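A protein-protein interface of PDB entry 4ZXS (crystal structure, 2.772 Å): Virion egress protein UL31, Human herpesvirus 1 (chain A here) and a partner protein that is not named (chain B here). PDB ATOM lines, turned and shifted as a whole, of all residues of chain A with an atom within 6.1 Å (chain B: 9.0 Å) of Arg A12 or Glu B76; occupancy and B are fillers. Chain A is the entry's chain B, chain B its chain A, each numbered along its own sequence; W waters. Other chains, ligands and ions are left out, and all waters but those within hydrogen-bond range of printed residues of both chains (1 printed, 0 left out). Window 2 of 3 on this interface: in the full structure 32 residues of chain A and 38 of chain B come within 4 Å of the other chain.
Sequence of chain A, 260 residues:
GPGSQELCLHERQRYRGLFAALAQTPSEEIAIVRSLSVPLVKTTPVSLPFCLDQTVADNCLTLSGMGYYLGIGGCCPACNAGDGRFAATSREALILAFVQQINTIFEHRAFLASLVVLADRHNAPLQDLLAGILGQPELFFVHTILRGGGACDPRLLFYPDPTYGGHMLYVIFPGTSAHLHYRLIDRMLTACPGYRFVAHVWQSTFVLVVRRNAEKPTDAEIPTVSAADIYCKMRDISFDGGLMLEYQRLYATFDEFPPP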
ATOM      1  N   LEU A   9       8.381  -4.146  26.770  1.00  0.00           N
ATOM      2  CA  LEU A   9       8.794  -5.493  27.140  1.00  0.00           C
ATOM      3  C   LEU A   9       7.645  -6.479  26.930  1.00  0.00           C
ATOM      4  O   LEU A   9       6.510  -6.071  26.701  1.00  0.00           O
ATOM      5  CB  LEU A   9       9.266  -5.507  28.599  1.00  0.00           C
ATOM      6  CG  LEU A   9      10.026  -6.715  29.149  1.00  0.00           C
ATOM      7  CD1 LEU A   9      11.277  -6.976  28.330  1.00  0.00           C
ATOM      8  CD2 LEU A   9      10.370  -6.507  30.617  1.00  0.00           C
ATOM      9  N   HIS A  10       7.941  -7.770  27.054  1.00  0.00           N
ATOM     10  CA  HIS A  10       6.965  -8.841  26.859  1.00  0.00           C
ATOM     11  C   HIS A  10       6.219  -8.705  25.530  1.00  0.00           C
ATOM     12  O   HIS A  10       4.988  -8.725  25.499  1.00  0.00           O
ATOM     13  CB  HIS A  10       5.958  -8.860  28.013  1.00  0.00           C
ATOM     14  CG  HIS A  10       6.554  -9.244  29.333  1.00  0.00           C
ATOM     15  ND1 HIS A  10       6.490  -8.427  30.437  1.00  0.00           N
ATOM     16  CD2 HIS A  10       7.218 -10.358  29.721  1.00  0.00           C
ATOM     17  CE1 HIS A  10       7.095  -9.021  31.457  1.00  0.00           C
ATOM     18  NE2 HIS A  10       7.543 -10.190  31.046  1.00  0.00           N
ATOM     19  N   GLU A  11       6.977  -8.560  24.444  1.00  0.00           N
ATOM     20  CA  GLU A  11       6.424  -8.445  23.092  1.00  0.00           C
ATOM     21  C   GLU A  11       5.438  -7.282  22.947  1.00  0.00           C
ATOM     22  O   GLU A  11       4.499  -7.350  22.153  1.00  0.00           O
ATOM     23  CB  GLU A  11       5.755  -9.762  22.684  1.00  0.00           C
ATOM     24  CG  GLU A  11       6.652 -10.982  22.860  1.00  0.00           C
ATOM     25  CD  GLU A  11       6.042 -12.252  22.296  1.00  0.00           C
ATOM     26  OE1 GLU A  11       4.857 -12.224  21.899  1.00  0.00           O
ATOM     27  OE2 GLU A  11       6.749 -13.281  22.250  1.00  0.00           O
ATOM     28  N   ARG A  12       5.657  -6.221  23.719  1.00  0.00           N
ATOM     29  CA  ARG A  12       4.810  -5.032  23.673  1.00  0.00           C
ATOM     30  C   ARG A  12       4.952  -4.309  22.338  1.00  0.00           C
ATOM     31  O   ARG A  12       4.010  -3.682  21.849  1.00  0.00           O
ATOM     32  CB  ARG A  12       5.158  -4.096  24.831  1.00  0.00           C
ATOM     33  CG  ARG A  12       4.263  -2.882  24.992  1.00  0.00           C
ATOM     34  CD  ARG A  12       4.612  -2.157  26.285  1.00  0.00           C
ATOM     35  NE  ARG A  12       3.720  -1.037  26.569  1.00  0.00           N
ATOM     36  CZ  ARG A  12       4.005   0.230  26.291  1.00  0.00           C
ATOM     37  NH1 ARG A  12       5.160   0.541  25.720  1.00  0.00           N
ATOM     38  NH2 ARG A  12       3.138   1.188  26.589  1.00  0.00           N
ATOM     39  N   GLN A  13       6.141  -4.415  21.756  1.00  0.00           N
ATOM     40  CA  GLN A  13       6.469  -3.746  20.503  1.00  0.00           C
ATOM     41  C   GLN A  13       5.607  -4.181  19.315  1.00  0.00           C
ATOM     42  O   GLN A  13       5.145  -3.342  18.545  1.00  0.00           O
ATOM     43  CB  GLN A  13       7.949  -3.979  20.176  1.00  0.00           C
ATOM     44  CG  GLN A  13       8.368  -5.445  20.230  1.00  0.00           C
ATOM     45  CD  GLN A  13       9.590  -5.743  19.387  1.00  0.00           C
ATOM     46  OE1 GLN A  13      10.342  -4.840  19.020  1.00  0.00           O
ATOM     47  NE2 GLN A  13       9.795  -7.018  19.072  1.00  0.00           N
ATOM     48  N   ARG A  14       5.379  -5.482  19.176  1.00  0.00           N
ATOM     49  CA  ARG A  14       4.671  -6.000  18.009  1.00  0.00           C
ATOM     50  C   ARG A  14       3.159  -5.802  18.122  1.00  0.00           C
ATOM     51  O   ARG A  14       2.455  -5.769  17.113  1.00  0.00           O
ATOM     52  CB  ARG A  14       4.998  -7.480  17.787  1.00  0.00           C
ATOM     53  CG  ARG A  14       4.283  -8.438  18.720  1.00  0.00           C
ATOM     54  CD  ARG A  14       4.493  -9.880  18.287  1.00  0.00           C
ATOM     55  NE  ARG A  14       5.878 -10.306  18.462  1.00  0.00           N
ATOM     56  CZ  ARG A  14       6.373 -11.445  17.992  1.00  0.00           C
ATOM     57  NH1 ARG A  14       5.598 -12.276  17.308  1.00  0.00           N
ATOM     58  NH2 ARG A  14       7.646 -11.754  18.200  1.00  0.00           N
ATOM     59  N   TYR A  15       2.666  -5.667  19.349  1.00  0.00           N
ATOM     60  CA  TYR A  15       1.233  -5.518  19.582  1.00  0.00           C
ATOM     61  C   TYR A  15       0.817  -4.055  19.705  1.00  0.00           C
ATOM     62  O   TYR A  15      -0.355  -3.722  19.522  1.00  0.00           O
ATOM     63  CB  TYR A  15       0.812  -6.280  20.841  1.00  0.00           C
ATOM     64  CG  TYR A  15       0.751  -7.779  20.659  1.00  0.00           C
ATOM     65  CD1 TYR A  15      -0.370  -8.387  20.110  1.00  0.00           C
ATOM     66  CD2 TYR A  15       1.808  -8.586  21.050  1.00  0.00           C
ATOM     67  CE1 TYR A  15      -0.429  -9.758  19.943  1.00  0.00           C
ATOM     68  CE2 TYR A  15       1.761  -9.958  20.887  1.00  0.00           C
ATOM     69  CZ  TYR A  15       0.639 -10.539  20.334  1.00  0.00           C
ATOM     70  OH  TYR A  15       0.586 -11.905  20.174  1.00  0.00           O
ATOM     71  N   ARG A  16       1.779  -3.195  20.037  1.00  0.00           N
ATOM     72  CA  ARG A  16       1.527  -1.767  20.223  1.00  0.00           C
ATOM     73  C   ARG A  16       0.778  -1.157  19.037  1.00  0.00           C
ATOM     74  O   ARG A  16      -0.245  -0.485  19.203  1.00  0.00           O
ATOM     75  CB  ARG A  16       2.851  -1.026  20.434  1.00  0.00           C
ATOM     76  CG  ARG A  16       2.730   0.487  20.546  1.00  0.00           C
ATOM     77  CD  ARG A  16       2.210   0.899  21.912  1.00  0.00           C
ATOM     78  NE  ARG A  16       2.161   2.349  22.071  1.00  0.00           N
ATOM     79  CZ  ARG A  16       1.999   2.966  23.238  1.00  0.00           C
ATOM     80  NH1 ARG A  16       1.880   2.256  24.352  1.00  0.00           N
ATOM     81  NH2 ARG A  16       1.962   4.290  23.293  1.00  0.00           N
ATOM     82  N   GLY A  17       1.295  -1.416  17.840  1.00  0.00           N
ATOM     83  CA  GLY A  17       0.714  -0.891  16.619  1.00  0.00           C
ATOM     84  C   GLY A  17      -0.693  -1.379  16.342  1.00  0.00           C
ATOM     85  O   GLY A  17      -1.590  -0.587  16.043  1.00  0.00           O
ATOM     86  N   ALA B  13      -8.346   7.947  31.452  1.00  0.00           N
ATOM     87  CA  ALA B  13      -7.743   6.928  30.597  1.00  0.00           C
ATOM     88  C   ALA B  13      -8.085   5.518  31.079  1.00  0.00           C
ATOM     89  O   ALA B  13      -8.413   4.635  30.278  1.00  0.00           O
ATOM     90  CB  ALA B  13      -6.234   7.115  30.537  1.00  0.00           C
ATOM     91  N   SER B  40      -2.685   6.477  36.708  1.00  0.00           N
ATOM     92  CA  SER B  40      -2.188   6.887  35.400  1.00  0.00           C
ATOM     93  C   SER B  40      -1.392   5.747  34.767  1.00  0.00           C
ATOM     94  O   SER B  40      -1.024   4.794  35.455  1.00  0.00           O
ATOM     95  CB  SER B  40      -1.320   8.142  35.535  1.00  0.00           C
ATOM     96  OG  SER B  40      -0.145   7.872  36.280  1.00  0.00           O
ATOM     97  N   PRO B  41      -1.134   5.827  33.450  1.00  0.00           N
ATOM     98  CA  PRO B  41      -0.255   4.837  32.820  1.00  0.00           C
ATOM     99  C   PRO B  41       1.169   4.874  33.373  1.00  0.00           C
ATOM    100  O   PRO B  41       1.927   3.921  33.194  1.00  0.00           O
ATOM    101  CB  PRO B  41      -0.276   5.244  31.344  1.00  0.00           C
ATOM    102  CG  PRO B  41      -1.577   5.937  31.169  1.00  0.00           C
ATOM    103  CD  PRO B  41      -1.792   6.686  32.451  1.00  0.00           C
ATOM    104  N   SER B  42       1.517   5.968  34.043  1.00  0.00           N
ATOM    105  CA  SER B  42       2.823   6.112  34.676  1.00  0.00           C
ATOM    106  C   SER B  42       2.907   5.354  36.000  1.00  0.00           C
ATOM    107  O   SER B  42       3.928   4.740  36.310  1.00  0.00           O
ATOM    108  CB  SER B  42       3.140   7.592  34.901  1.00  0.00           C
ATOM    109  OG  SER B  42       4.359   7.751  35.605  1.00  0.00           O
ATOM    110  N   SER B  43       1.829   5.401  36.777  1.00  0.00           N
ATOM    111  CA  SER B  43       1.803   4.772  38.094  1.00  0.00           C
ATOM    112  C   SER B  43       0.801   3.621  38.162  1.00  0.00           C
ATOM    113  O   SER B  43      -0.402   3.820  37.991  1.00  0.00           O
ATOM    114  CB  SER B  43       1.474   5.810  39.169  1.00  0.00           C
ATOM    115  OG  SER B  43       0.373   6.612  38.778  1.00  0.00           O
ATOM    116  N   LEU B  44       1.304   2.418  38.422  1.00  0.00           N
ATOM    117  CA  LEU B  44       0.463   1.225  38.463  1.00  0.00           C
ATOM    118  C   LEU B  44       0.247   0.741  39.894  1.00  0.00           C
ATOM    119  O   LEU B  44       1.196   0.648  40.674  1.00  0.00           O
ATOM    120  CB  LEU B  44       1.083   0.106  37.623  1.00  0.00           C
ATOM    121  CG  LEU B  44       1.431   0.443  36.173  1.00  0.00           C
ATOM    122  CD1 LEU B  44       2.134  -0.727  35.504  1.00  0.00           C
ATOM    123  CD2 LEU B  44       0.180   0.831  35.400  1.00  0.00           C
ATOM    124  N   LEU B  68      -4.532  -9.159  29.012  1.00  0.00           N
ATOM    125  CA  LEU B  68      -3.223  -8.914  29.614  1.00  0.00           C
ATOM    126  C   LEU B  68      -2.356  -8.060  28.693  1.00  0.00           C
ATOM    127  O   LEU B  68      -1.653  -7.153  29.144  1.00  0.00           O
ATOM    128  CB  LEU B  68      -2.512 -10.233  29.929  1.00  0.00           C
ATOM    129  CG  LEU B  68      -3.108 -11.159  30.992  1.00  0.00           C
ATOM    130  CD1 LEU B  68      -2.153 -12.304  31.298  1.00  0.00           C
ATOM    131  CD2 LEU B  68      -3.453 -10.401  32.261  1.00  0.00           C
ATOM    132  N   ARG B  69      -2.420  -8.358  27.399  1.00  0.00           N
ATOM    133  CA  ARG B  69      -1.672  -7.611  26.398  1.00  0.00           C
ATOM    134  C   ARG B  69      -2.186  -6.182  26.277  1.00  0.00           C
ATOM    135  O   ARG B  69      -1.409  -5.256  26.054  1.00  0.00           O
ATOM    136  CB  ARG B  69      -1.739  -8.315  25.043  1.00  0.00           C
ATOM    137  CG  ARG B  69      -0.987  -9.634  24.996  1.00  0.00           C
ATOM    138  CD  ARG B  69      -0.527  -9.956  23.586  1.00  0.00           C
ATOM    139  NE  ARG B  69       0.049 -11.293  23.491  1.00  0.00           N
ATOM    140  CZ  ARG B  69       1.311 -11.584  23.791  1.00  0.00           C
ATOM    141  NH1 ARG B  69       2.131 -10.630  24.209  1.00  0.00           N
ATOM    142  NH2 ARG B  69       1.752 -12.828  23.673  1.00  0.00           N
ATOM    143  N   LEU B  70      -3.497  -6.008  26.421  1.00  0.00           N
ATOM    144  CA  LEU B  70      -4.085  -4.673  26.411  1.00  0.00           C
ATOM    145  C   LEU B  70      -3.570  -3.854  27.590  1.00  0.00           C
ATOM    146  O   LEU B  70      -3.202  -2.684  27.437  1.00  0.00           O
ATOM    147  CB  LEU B  70      -5.614  -4.747  26.442  1.00  0.00           C
ATOM    148  CG  LEU B  70      -6.311  -4.770  25.080  1.00  0.00           C
ATOM    149  CD1 LEU B  70      -7.821  -4.835  25.245  1.00  0.00           C
ATOM    150  CD2 LEU B  70      -5.913  -3.551  24.260  1.00  0.00           C
ATOM    151  N   MET B  71      -3.535  -4.477  28.765  1.00  0.00           N
ATOM    152  CA  MET B  71      -3.026  -3.810  29.957  1.00  0.00           C
ATOM    153  C   MET B  71      -1.550  -3.449  29.819  1.00  0.00           C
ATOM    154  O   MET B  71      -1.139  -2.348  30.183  1.00  0.00           O
ATOM    155  CB  MET B  71      -3.229  -4.682  31.195  1.00  0.00           C
ATOM    156  CG  MET B  71      -4.678  -4.941  31.550  1.00  0.00           C
ATOM    157  SD  MET B  71      -4.822  -5.489  33.257  1.00  0.00           S
ATOM    158  CE  MET B  71      -3.810  -6.963  33.214  1.00  0.00           C
ATOM    159  N   ASN B  72      -0.756  -4.376  29.290  1.00  0.00           N
ATOM    160  CA  ASN B  72       0.671  -4.131  29.106  1.00  0.00           C
ATOM    161  C   ASN B  72       0.914  -3.042  28.066  1.00  0.00           C
ATOM    162  O   ASN B  72       1.891  -2.296  28.147  1.00  0.00           O
ATOM    163  CB  ASN B  72       1.394  -5.415  28.699  1.00  0.00           C
ATOM    164  CG  ASN B  72       2.904  -5.269  28.731  1.00  0.00           C
ATOM    165  OD1 ASN B  72       3.438  -4.377  29.391  1.00  0.00           O
ATOM    166  ND2 ASN B  72       3.599  -6.148  28.020  1.00  0.00           N
ATOM    167  N   ASP B  73       0.010  -2.954  27.097  1.00  0.00           N
ATOM    168  CA  ASP B  73       0.078  -1.930  26.063  1.00  0.00           C
ATOM    169  C   ASP B  73      -0.260  -0.560  26.636  1.00  0.00           C
ATOM    170  O   ASP B  73       0.322   0.451  26.244  1.00  0.00           O
ATOM    171  CB  ASP B  73      -0.874  -2.268  24.915  1.00  0.00           C
ATOM    172  CG  ASP B  73      -0.876  -1.212  23.828  1.00  0.00           C
ATOM    173  OD1 ASP B  73       0.104  -1.151  23.060  1.00  0.00           O
ATOM    174  OD2 ASP B  73      -1.856  -0.442  23.743  1.00  0.00           O
ATOM    175  N   TRP B  74      -1.209  -0.538  27.567  1.00  0.00           N
ATOM    176  CA  TRP B  74      -1.682   0.710  28.155  1.00  0.00           C
ATOM    177  C   TRP B  74      -0.635   1.372  29.056  1.00  0.00           C
ATOM    178  O   TRP B  74      -0.532   2.597  29.104  1.00  0.00           O
ATOM    179  CB  TRP B  74      -2.970   0.457  28.940  1.00  0.00           C
ATOM    180  CG  TRP B  74      -3.598   1.692  29.505  1.00  0.00           C
ATOM    181  CD1 TRP B  74      -4.407   2.572  28.847  1.00  0.00           C
ATOM    182  CD2 TRP B  74      -3.492   2.172  30.849  1.00  0.00           C
ATOM    183  NE1 TRP B  74      -4.800   3.578  29.696  1.00  0.00           N
ATOM    184  CE2 TRP B  74      -4.253   3.355  30.932  1.00  0.00           C
ATOM    185  CE3 TRP B  74      -2.824   1.720  31.991  1.00  0.00           C
ATOM    186  CZ2 TRP B  74      -4.365   4.091  32.109  1.00  0.00           C
ATOM    187  CZ3 TRP B  74      -2.935   2.452  33.159  1.00  0.00           C
ATOM    188  CH2 TRP B  74      -3.698   3.624  33.208  1.00  0.00           C
ATOM    189  N   ALA B  75       0.138   0.555  29.767  1.00  0.00           N
ATOM    190  CA  ALA B  75       1.148   1.056  30.698  1.00  0.00           C
ATOM    191  C   ALA B  75       2.370   1.637  29.985  1.00  0.00           C
ATOM    192  O   ALA B  75       2.825   1.099  28.977  1.00  0.00           O
ATOM    193  CB  ALA B  75       1.576  -0.052  31.649  1.00  0.00           C
ATOM    194  N   GLU B  76       2.895   2.738  30.519  1.00  0.00           N
ATOM    195  CA  GLU B  76       4.083   3.379  29.957  1.00  0.00           C
ATOM    196  C   GLU B  76       5.327   3.037  30.771  1.00  0.00           C
ATOM    197  O   GLU B  76       6.426   3.499  30.469  1.00  0.00           O
ATOM    198  CB  GLU B  76       3.903   4.899  29.902  1.00  0.00           C
ATOM    199  CG  GLU B  76       2.589   5.369  29.290  1.00  0.00           C
ATOM    200  CD  GLU B  76       2.611   5.411  27.773  1.00  0.00           C
ATOM    201  OE1 GLU B  76       3.208   4.509  27.150  1.00  0.00           O
ATOM    202  OE2 GLU B  76       2.022   6.353  27.203  1.00  0.00           O
ATOM    203  N   VAL B  77       5.142   2.222  31.802  1.00  0.00           N
ATOM    204  CA  VAL B  77       6.239   1.767  32.648  1.00  0.00           C
ATOM    205  C   VAL B  77       6.288   0.240  32.593  1.00  0.00           C
ATOM    206  O   VAL B  77       5.239  -0.406  32.544  1.00  0.00           O
ATOM    207  CB  VAL B  77       6.063   2.274  34.106  1.00  0.00           C
ATOM    208  CG1 VAL B  77       4.679   1.921  34.636  1.00  0.00           C
ATOM    209  CG2 VAL B  77       7.151   1.743  35.030  1.00  0.00           C
ATOM    210  N   PRO B  78       7.500  -0.346  32.581  1.00  0.00           N
ATOM    211  CA  PRO B  78       7.609  -1.806  32.484  1.00  0.00           C
ATOM    212  C   PRO B  78       6.860  -2.540  33.594  1.00  0.00           C
ATOM    213  O   PRO B  78       6.869  -2.109  34.747  1.00  0.00           O
ATOM    214  CB  PRO B  78       9.115  -2.048  32.598  1.00  0.00           C
ATOM    215  CG  PRO B  78       9.721  -0.823  32.013  1.00  0.00           C
ATOM    216  CD  PRO B  78       8.803   0.315  32.378  1.00  0.00           C
ATOM    217  N   CYS B  79       6.217  -3.646  33.228  1.00  0.00           N
ATOM    218  CA  CYS B  79       5.400  -4.416  34.156  1.00  0.00           C
ATOM    219  C   CYS B  79       5.074  -5.787  33.577  1.00  0.00           C
ATOM    220  O   CYS B  79       5.192  -6.004  32.371  1.00  0.00           O
ATOM    221  CB  CYS B  79       4.107  -3.667  34.482  1.00  0.00           C
ATOM    222  SG  CYS B  79       2.969  -3.498  33.083  1.00  0.00           S
ATOM    223  N   PRO B  81       1.863  -7.994  33.596  1.00  0.00           N
ATOM    224  CA  PRO B  81       0.428  -8.163  33.855  1.00  0.00           C
ATOM    225  C   PRO B  81       0.070  -9.576  34.306  1.00  0.00           C
ATOM    226  O   PRO B  81       0.623 -10.550  33.795  1.00  0.00           O
ATOM    227  CB  PRO B  81      -0.208  -7.843  32.503  1.00  0.00           C
ATOM    228  CG  PRO B  81       0.734  -6.881  31.886  1.00  0.00           C
ATOM    229  CD  PRO B  81       2.105  -7.347  32.295  1.00  0.00           C
ATOM    230  N   PHE B  98      -1.576  -5.405  37.241  1.00  0.00           N
ATOM    231  CA  PHE B  98      -0.425  -4.988  36.447  1.00  0.00           C
ATOM    232  C   PHE B  98       0.817  -5.681  36.986  1.00  0.00           C
ATOM    233  O   PHE B  98       1.780  -5.922  36.256  1.00  0.00           O
ATOM    234  CB  PHE B  98      -0.263  -3.467  36.473  1.00  0.00           C
ATOM    235  CG  PHE B  98      -1.263  -2.738  35.621  1.00  0.00           C
ATOM    236  CD1 PHE B  98      -1.123  -2.704  34.242  1.00  0.00           C
ATOM    237  CD2 PHE B  98      -2.345  -2.091  36.194  1.00  0.00           C
ATOM    238  CE1 PHE B  98      -2.042  -2.035  33.452  1.00  0.00           C
ATOM    239  CE2 PHE B  98      -3.267  -1.421  35.410  1.00  0.00           C
ATOM    240  CZ  PHE B  98      -3.115  -1.393  34.038  1.00  0.00           C
ATOM    241  N   LEU B 128       1.719 -12.527  31.903  1.00  0.00           N
ATOM    242  CA  LEU B 128       1.915 -12.428  30.462  1.00  0.00           C
ATOM    243  C   LEU B 128       3.278 -12.976  30.049  1.00  0.00           C
ATOM    244  O   LEU B 128       3.438 -13.492  28.945  1.00  0.00           O
ATOM    245  CB  LEU B 128       1.760 -10.979  29.992  1.00  0.00           C
ATOM    246  CG  LEU B 128       1.718 -10.797  28.472  1.00  0.00           C
ATOM    247  CD1 LEU B 128       0.601 -11.638  27.869  1.00  0.00           C
ATOM    248  CD2 LEU B 128       1.551  -9.331  28.103  1.00  0.00           C
ATOM    249  N   ASP B 132       3.721 -15.977  27.500  1.00  0.00           N
ATOM    250  CA  ASP B 132       4.575 -15.845  26.326  1.00  0.00           C
ATOM    251  C   ASP B 132       5.613 -16.957  26.285  1.00  0.00           C
ATOM    252  O   ASP B 132       5.946 -17.465  25.215  1.00  0.00           O
ATOM    253  CB  ASP B 132       5.267 -14.481  26.313  1.00  0.00           C
ATOM    254  CG  ASP B 132       4.433 -13.409  25.642  1.00  0.00           C
ATOM    255  OD1 ASP B 132       3.557 -13.761  24.824  1.00  0.00           O
ATOM    256  OD2 ASP B 132       4.657 -12.215  25.929  1.00  0.00           O
HETATM  257  O   HOH W   1       2.553 -13.297  20.408  1.00  0.00           O
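The backbone carbonyl oxygen (O) of Pro B41 is in hydrogen-bond range of the backbone NH (N) of Glu B76 (3.1 Å). The side-chain carboxylate (OD2) of Asp B132 lies within salt-bridge range of the guanidinium group (NH1) of Arg B69 (3.4 Å).
The guanidinium group (NH2) of Arg B69 is in salt-bridge range of the side-chain carboxylate (OE1) of Glu A11 (3.6 Å). The side-chain hydroxyl (OH) of Tyr A15 sits close to the guanidinium group (NE) of Arg B69. ND2 of Asn B72 lies within hydrogen-bond range of O of Leu A9 (3.2 Å). The backbone carbonyl oxygen (O) of Asn B72 lies within hydrogen-bond range of the guanidinium group (NE) of Arg A12 (2.7 Å). The backbone carbonyl oxygen of Asp B73 is in hydrogen-bond range of the guanidinium group of Arg A12 (2.9 Å). The guanidinium group (NH1) of Arg A16 sits at hydrogen-bond distance from the backbone carbonyl oxygen (O) of Asp B73 (3.0 Å). The backbone carbonyl oxygen (O) of Ala B75 sits at hydrogen-bond distance from the guanidinium group (NH2) of Arg A12 (2.4 Å). The guanidinium group of Arg A12 lies within salt-bridge range of the side-chain carboxylate of Glu B76 (3.4 Å). The side-chain carboxylate (OE1) of Glu B76 is in salt-bridge range of the guanidinium group (NH1) of Arg A16 (3.8 Å). ND1 of His A10 sits at hydrogen-bond distance from O of Cys B79.
Arg A12 touches just these residues of chain B: Asn B72, Asp B73, Ala B75 and Glu B76. Of chain A, only Arg A12 (3.4 Å) and Arg A16 (3.8 Å) come within 4 Å of Glu B76. Of the printed residues of chain B, Glu A11 touches Arg B69 (3.6 Å) and Asp B132 (3.6 Å). Of the printed residues of chain A, Asp B73 touches Arg A12 (2.9 Å) and Arg A16 (3.0 Å). Of the printed residues of chain A, Cys B79 touches His A10 (3.4 Å). Of the printed residues of chain B, Leu A9 touches Asn B72 (3.2 Å). Printed residues of chain A within 4 Å of Arg B69: His A10 (3.7 Å), Glu A11 (3.6 Å) and Tyr A15 (3.3 Å). Pro B41 touches none of the printed residues of chain A. The nearest printed residue of chain A that does not touch Glu B76 is Leu A9 (8.7 Å). The nearest printed residue of chain A that does not touch Asp B132 is Tyr A15 (5.8 Å).
Of the 9 printed residues of chain A, 6 touch a printed residue of chain B. Printed residues of chain A that touch a printed residue of chain B: Leu A9, His A10, Glu A11, Arg A12, Tyr A15 and Arg A16. Hydrophobic or aromatic side chains of chain A within 4 Å of the printed part of chain B: His A10 and Tyr A15. Among the printed residues, Asp or Glu carboxylates within 4 Å of a Lys or Arg side-chain nitrogen of the other chain: Glu A11 with Arg B69 (3.6 Å), Arg A12 with Glu B76 (3.4 Å) and Arg A16 with Glu B76 (3.8 Å).
His A10 touches Arg B69 (O to NH1, 3.7 Å). His A10 touches Asn B72 (CB to ND2, 3.6 Å). Asp B132 touches His A10 (OD2 to O, 3.5 Å). OD1 of Asp B132 touches OE1 of Glu A11, at 3.6 Å.
Water W1 lies within hydrogen-bond range of OH of Tyr A15 (2.4 Å), OE1 of Glu A11 (2.9 Å) and NH2 of Arg B69 (3.4 Å).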
